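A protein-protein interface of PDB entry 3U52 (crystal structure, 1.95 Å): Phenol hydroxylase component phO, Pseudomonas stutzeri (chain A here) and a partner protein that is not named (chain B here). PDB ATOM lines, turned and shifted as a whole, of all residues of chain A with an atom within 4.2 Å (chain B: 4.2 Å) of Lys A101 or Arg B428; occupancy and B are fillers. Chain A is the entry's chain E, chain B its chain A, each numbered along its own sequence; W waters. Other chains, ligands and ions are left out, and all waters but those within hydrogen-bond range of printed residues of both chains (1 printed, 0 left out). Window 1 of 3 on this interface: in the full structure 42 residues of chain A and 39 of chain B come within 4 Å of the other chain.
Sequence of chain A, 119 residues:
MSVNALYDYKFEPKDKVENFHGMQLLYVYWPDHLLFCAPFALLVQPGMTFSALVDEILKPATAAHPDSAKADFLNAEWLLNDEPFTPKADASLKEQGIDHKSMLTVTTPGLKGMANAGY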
ATOM      1  N   ASP A  15     -22.827 -15.096 -24.267  1.00  0.00           N
ATOM      2  CA  ASP A  15     -21.372 -15.224 -24.123  1.00  0.00           C
ATOM      3  C   ASP A  15     -20.918 -15.916 -22.825  1.00  0.00           C
ATOM      4  O   ASP A  15     -19.832 -15.637 -22.317  1.00  0.00           O
ATOM      5  CB  ASP A  15     -20.653 -13.868 -24.259  1.00  0.00           C
ATOM      6  CG  ASP A  15     -20.955 -13.170 -25.598  1.00  0.00           C
ATOM      7  OD1 ASP A  15     -21.210 -11.925 -25.597  1.00  0.00           O
ATOM      8  OD2 ASP A  15     -20.895 -13.865 -26.639  1.00  0.00           O
ATOM      9  N   LEU A  25     -12.550 -15.557 -22.564  1.00  0.00           N
ATOM     10  CA  LEU A  25     -12.275 -14.142 -22.962  1.00  0.00           C
ATOM     11  C   LEU A  25     -11.504 -13.416 -21.867  1.00  0.00           C
ATOM     12  O   LEU A  25     -11.801 -13.548 -20.681  1.00  0.00           O
ATOM     13  CB  LEU A  25     -13.597 -13.377 -23.215  1.00  0.00           C
ATOM     14  CG  LEU A  25     -14.332 -13.768 -24.517  1.00  0.00           C
ATOM     15  CD1 LEU A  25     -15.720 -13.169 -24.508  1.00  0.00           C
ATOM     16  CD2 LEU A  25     -13.514 -13.409 -25.776  1.00  0.00           C
ATOM     17  N   TYR A  27      -9.782  -9.328 -21.354  1.00  0.00           N
ATOM     18  CA  TYR A  27      -9.582  -7.996 -21.915  1.00  0.00           C
ATOM     19  C   TYR A  27      -8.406  -7.364 -21.264  1.00  0.00           C
ATOM     20  O   TYR A  27      -8.254  -7.487 -20.059  1.00  0.00           O
ATOM     21  CB  TYR A  27     -10.812  -7.104 -21.631  1.00  0.00           C
ATOM     22  CG  TYR A  27     -12.124  -7.641 -22.156  1.00  0.00           C
ATOM     23  CD1 TYR A  27     -12.381  -7.707 -23.534  1.00  0.00           C
ATOM     24  CD2 TYR A  27     -13.101  -8.088 -21.283  1.00  0.00           C
ATOM     25  CE1 TYR A  27     -13.598  -8.216 -24.012  1.00  0.00           C
ATOM     26  CE2 TYR A  27     -14.305  -8.616 -21.751  1.00  0.00           C
ATOM     27  CZ  TYR A  27     -14.544  -8.680 -23.109  1.00  0.00           C
ATOM     28  OH  TYR A  27     -15.777  -9.179 -23.549  1.00  0.00           O
ATOM     29  N   ASN A  81     -10.090  -6.496 -12.693  1.00  0.00           N
ATOM     30  CA  ASN A  81     -11.467  -6.109 -12.405  1.00  0.00           C
ATOM     31  C   ASN A  81     -11.562  -4.883 -11.474  1.00  0.00           C
ATOM     32  O   ASN A  81     -12.446  -4.799 -10.617  1.00  0.00           O
ATOM     33  CB  ASN A  81     -12.301  -7.327 -11.933  1.00  0.00           C
ATOM     34  CG  ASN A  81     -12.282  -8.438 -12.965  1.00  0.00           C
ATOM     35  OD1 ASN A  81     -12.376  -8.136 -14.155  1.00  0.00           O
ATOM     36  ND2 ASN A  81     -12.081  -9.718 -12.541  1.00  0.00           N
ATOM     37  N   ASP A  99     -10.673 -14.889 -14.440  1.00  0.00           N
ATOM     38  CA  ASP A  99     -11.785 -15.690 -14.940  1.00  0.00           C
ATOM     39  C   ASP A  99     -12.359 -15.087 -16.258  1.00  0.00           C
ATOM     40  O   ASP A  99     -11.814 -14.101 -16.788  1.00  0.00           O
ATOM     41  CB  ASP A  99     -12.856 -15.850 -13.864  1.00  0.00           C
ATOM     42  CG  ASP A  99     -13.563 -14.548 -13.511  1.00  0.00           C
ATOM     43  OD1 ASP A  99     -13.546 -13.539 -14.300  1.00  0.00           O
ATOM     44  OD2 ASP A  99     -14.194 -14.547 -12.423  1.00  0.00           O
ATOM     45  N   HIS A 100     -13.399 -15.716 -16.793  1.00  0.00           N
ATOM     46  CA  HIS A 100     -13.911 -15.374 -18.135  1.00  0.00           C
ATOM     47  C   HIS A 100     -14.439 -13.933 -18.123  1.00  0.00           C
ATOM     48  O   HIS A 100     -15.126 -13.527 -17.198  1.00  0.00           O
ATOM     49  CB  HIS A 100     -14.967 -16.405 -18.535  1.00  0.00           C
ATOM     50  CG  HIS A 100     -15.665 -16.134 -19.821  1.00  0.00           C
ATOM     51  ND1 HIS A 100     -15.031 -16.147 -21.041  1.00  0.00           N
ATOM     52  CD2 HIS A 100     -16.973 -15.874 -20.071  1.00  0.00           C
ATOM     53  CE1 HIS A 100     -15.923 -15.921 -21.997  1.00  0.00           C
ATOM     54  NE2 HIS A 100     -17.107 -15.742 -21.431  1.00  0.00           N
ATOM     55  N   LYS A 101     -14.057 -13.170 -19.135  1.00  0.00           N
ATOM     56  CA  LYS A 101     -14.420 -11.748 -19.242  1.00  0.00           C
ATOM     57  C   LYS A 101     -13.909 -10.805 -18.114  1.00  0.00           C
ATOM     58  O   LYS A 101     -14.443  -9.711 -17.888  1.00  0.00           O
ATOM     59  CB  LYS A 101     -15.935 -11.620 -19.492  1.00  0.00           C
ATOM     60  CG  LYS A 101     -16.331 -11.919 -20.949  1.00  0.00           C
ATOM     61  CD  LYS A 101     -17.724 -11.322 -21.266  1.00  0.00           C
ATOM     62  CE  LYS A 101     -18.796 -12.338 -20.830  1.00  0.00           C
ATOM     63  NZ  LYS A 101     -20.124 -11.687 -20.745  1.00  0.00           N
ATOM     64  N   SER A 102     -12.859 -11.223 -17.420  1.00  0.00           N
ATOM     65  CA  SER A 102     -12.066 -10.294 -16.595  1.00  0.00           C
ATOM     66  C   SER A 102     -11.382  -9.246 -17.473  1.00  0.00           C
ATOM     67  O   SER A 102     -11.044  -9.495 -18.652  1.00  0.00           O
ATOM     68  CB  SER A 102     -11.005 -11.057 -15.771  1.00  0.00           C
ATOM     69  OG  SER A 102     -11.662 -11.663 -14.666  1.00  0.00           O
ATOM     70  N   MET A 103     -11.127  -8.097 -16.877  1.00  0.00           N
ATOM     71  CA  MET A 103     -10.249  -7.111 -17.520  1.00  0.00           C
ATOM     72  C   MET A 103      -9.078  -6.864 -16.618  1.00  0.00           C
ATOM     73  O   MET A 103      -9.266  -6.501 -15.471  1.00  0.00           O
ATOM     74  CB  MET A 103     -10.964  -5.784 -17.774  1.00  0.00           C
ATOM     75  CG  MET A 103     -10.090  -4.821 -18.623  1.00  0.00           C
ATOM     76  SD  MET A 103     -10.914  -3.405 -19.205  1.00  0.00           S
ATOM     77  CE  MET A 103     -11.207  -3.891 -20.856  1.00  0.00           C
ATOM     78  N   ILE B 422     -19.546  -4.605 -14.724  1.00  0.00           N
ATOM     79  CA  ILE B 422     -20.483  -5.009 -13.705  1.00  0.00           C
ATOM     80  C   ILE B 422     -20.422  -6.536 -13.638  1.00  0.00           C
ATOM     81  O   ILE B 422     -19.863  -7.174 -14.527  1.00  0.00           O
ATOM     82  CB  ILE B 422     -21.883  -4.394 -14.054  1.00  0.00           C
ATOM     83  CG1 ILE B 422     -22.419  -3.458 -12.950  1.00  0.00           C
ATOM     84  CG2 ILE B 422     -22.819  -5.343 -14.848  1.00  0.00           C
ATOM     85  CD1 ILE B 422     -23.435  -4.061 -11.901  1.00  0.00           C
ATOM     86  N   GLU B 423     -20.912  -7.092 -12.535  1.00  0.00           N
ATOM     87  CA  GLU B 423     -21.208  -8.507 -12.423  1.00  0.00           C
ATOM     88  C   GLU B 423     -22.711  -8.636 -12.386  1.00  0.00           C
ATOM     89  O   GLU B 423     -23.395  -7.914 -11.644  1.00  0.00           O
ATOM     90  CB  GLU B 423     -20.627  -9.073 -11.136  1.00  0.00           C
ATOM     91  CG  GLU B 423     -19.159  -8.977 -11.091  1.00  0.00           C
ATOM     92  CD  GLU B 423     -18.602  -9.580  -9.836  1.00  0.00           C
ATOM     93  OE1 GLU B 423     -18.709 -10.835  -9.676  1.00  0.00           O
ATOM     94  OE2 GLU B 423     -18.057  -8.802  -9.014  1.00  0.00           O
ATOM     95  N   GLU B 427     -21.771 -13.467 -14.104  1.00  0.00           N
ATOM     96  CA  GLU B 427     -21.086 -13.228 -15.385  1.00  0.00           C
ATOM     97  C   GLU B 427     -20.620 -11.767 -15.409  1.00  0.00           C
ATOM     98  O   GLU B 427     -21.221 -10.952 -14.772  1.00  0.00           O
ATOM     99  CB  GLU B 427     -22.048 -13.475 -16.576  1.00  0.00           C
ATOM    100  CG  GLU B 427     -22.408 -15.000 -16.862  1.00  0.00           C
ATOM    101  CD  GLU B 427     -21.272 -15.753 -17.538  1.00  0.00           C
ATOM    102  OE1 GLU B 427     -20.435 -15.098 -18.218  1.00  0.00           O
ATOM    103  OE2 GLU B 427     -21.179 -17.006 -17.400  1.00  0.00           O
ATOM    104  N   ARG B 428     -19.585 -11.427 -16.160  1.00  0.00           N
ATOM    105  CA  ARG B 428     -19.078 -10.054 -16.146  1.00  0.00           C
ATOM    106  C   ARG B 428     -19.516  -9.425 -17.480  1.00  0.00           C
ATOM    107  O   ARG B 428     -19.522 -10.116 -18.504  1.00  0.00           O
ATOM    108  CB  ARG B 428     -17.562 -10.003 -16.045  1.00  0.00           C
ATOM    109  CG  ARG B 428     -16.945 -10.877 -14.875  1.00  0.00           C
ATOM    110  CD  ARG B 428     -15.451 -10.574 -14.750  1.00  0.00           C
ATOM    111  NE  ARG B 428     -14.924 -11.286 -13.596  1.00  0.00           N
ATOM    112  CZ  ARG B 428     -15.062 -10.889 -12.326  1.00  0.00           C
ATOM    113  NH1 ARG B 428     -15.664  -9.759 -12.013  1.00  0.00           N
ATOM    114  NH2 ARG B 428     -14.557 -11.642 -11.356  1.00  0.00           N
ATOM    115  N   TYR B 429     -19.864  -8.153 -17.447  1.00  0.00           N
ATOM    116  CA  TYR B 429     -20.308  -7.420 -18.665  1.00  0.00           C
ATOM    117  C   TYR B 429     -19.616  -6.093 -18.630  1.00  0.00           C
ATOM    118  O   TYR B 429     -19.372  -5.569 -17.532  1.00  0.00           O
ATOM    119  CB  TYR B 429     -21.824  -7.205 -18.711  1.00  0.00           C
ATOM    120  CG  TYR B 429     -22.534  -8.530 -18.772  1.00  0.00           C
ATOM    121  CD1 TYR B 429     -22.635  -9.245 -19.963  1.00  0.00           C
ATOM    122  CD2 TYR B 429     -23.051  -9.101 -17.595  1.00  0.00           C
ATOM    123  CE1 TYR B 429     -23.266 -10.528 -19.999  1.00  0.00           C
ATOM    124  CE2 TYR B 429     -23.639 -10.376 -17.604  1.00  0.00           C
ATOM    125  CZ  TYR B 429     -23.728 -11.075 -18.801  1.00  0.00           C
ATOM    126  OH  TYR B 429     -24.362 -12.285 -18.790  1.00  0.00           O
ATOM    127  N   HIS B 430     -19.331  -5.558 -19.819  1.00  0.00           N
ATOM    128  CA  HIS B 430     -18.579  -4.306 -19.979  1.00  0.00           C
ATOM    129  C   HIS B 430     -19.335  -3.298 -20.871  1.00  0.00           C
ATOM    130  O   HIS B 430     -20.055  -3.688 -21.825  1.00  0.00           O
ATOM    131  CB  HIS B 430     -17.203  -4.581 -20.594  1.00  0.00           C
ATOM    132  CG  HIS B 430     -16.396  -5.578 -19.807  1.00  0.00           C
ATOM    133  ND1 HIS B 430     -15.445  -5.197 -18.888  1.00  0.00           N
ATOM    134  CD2 HIS B 430     -16.493  -6.927 -19.713  1.00  0.00           C
ATOM    135  CE1 HIS B 430     -14.938  -6.276 -18.310  1.00  0.00           C
ATOM    136  NE2 HIS B 430     -15.559  -7.337 -18.790  1.00  0.00           N
HETATM  137  O   HOH W   1     -18.477 -13.687 -17.388  1.00  0.00           O
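Of the 9 printed residues of chain A, 6 touch a printed residue of chain B. Printed residues of chain A that touch a printed residue of chain B: Tyr A27, Asn A81, Asp A99, His A100, Lys A101 and Ser A102. Hydrophobic or aromatic side chains of chain A that line the printed part of chain B: Tyr A27. Of the 6 printed residues of chain B, 3 touch a printed residue of chain A. Hydrophobic or aromatic side chains of chain B that line the printed part of chain A: Tyr B429 and His B430. Along chain B the printed residues that touch a printed residue of chain A span positions 428 to 430. Among the printed residues, 8 pairs touch across the chains. Among the printed residues, Asp or Glu carboxylates within 4 Å of a Lys or Arg side-chain nitrogen of the other chain: Asp A99 with Arg B428.
The guanidinium group (NH2) of Arg B428 lies close to the side-chain amide nitrogen (ND2) of Asn A81 (3.4 Å). NE of Arg B428 lies within salt-bridge range of OD1 of Asp A99, 2.7 Å away. O of Arg B428 is in hydrogen-bond range of NZ of Lys A101, at 2.8 Å. NE of Arg B428 is in hydrogen-bond range of OG of Ser A102, at 3.5 Å. O of Lys A101 is in hydrogen-bond range of NE2 of His B430, at 2.8 Å.
The guanidinium group (NH1) of Arg B428 lies within salt-bridge range of the side-chain carboxylate (OE2) of Glu B423. N of Leu A25 sits at hydrogen-bond distance from ND1 of His A100 (3.0 Å). N of Tyr A27 sits at hydrogen-bond distance from O of Ser A102 (3.0 Å). The side-chain amide nitrogen of Asn A81 sits at hydrogen-bond distance from the side-chain hydroxyl of Ser A102, at 2.9 Å. O of Met A103 is in hydrogen-bond range of N of Asn A81 (2.9 Å). OD1 of Asp A99 sits at hydrogen-bond distance from OG of Ser A102, 2.7 Å away.
Among the printed residues, pairs that only touch across the chains: Tyr A27 with His B430 (3.4 Å), His A100 with Arg B428 (3.8 Å) and Lys A101 with Tyr B429 (3.4 Å).
Water W1 lies within hydrogen-bond range of OE1 of Glu B427 (2.6 Å), N of Arg B428 (2.8 Å) and O of His A100 (3.4 Å).
Printed residues of chain B within 4 Å of Tyr A27: His B430 (3.4 Å). Printed residues of chain B within 4 Å of Asn A81: Arg B428. Of the printed residues of chain B, Asp A99 touches Arg B428. Printed residues of chain B within 4 Å of His A100: Arg B428 (3.8 Å). Lys A101 touches just these residues of chain B: Arg B428 (2.8 Å), Tyr B429 (3.4 Å) and His B430 (2.8 Å). Of the printed residues of chain A, Arg B428 touches Asn A81 (3.2 Å), Asp A99 (2.7 Å), His A100 (3.8 Å), Lys A101 (2.8 Å) and Ser A102 (3.5 Å). Printed residues of chain A within 4 Å of His B430: Tyr A27 and Lys A101. The nearest printed residue of chain A that does not touch His B430 is Met A103 (4.04 Å).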
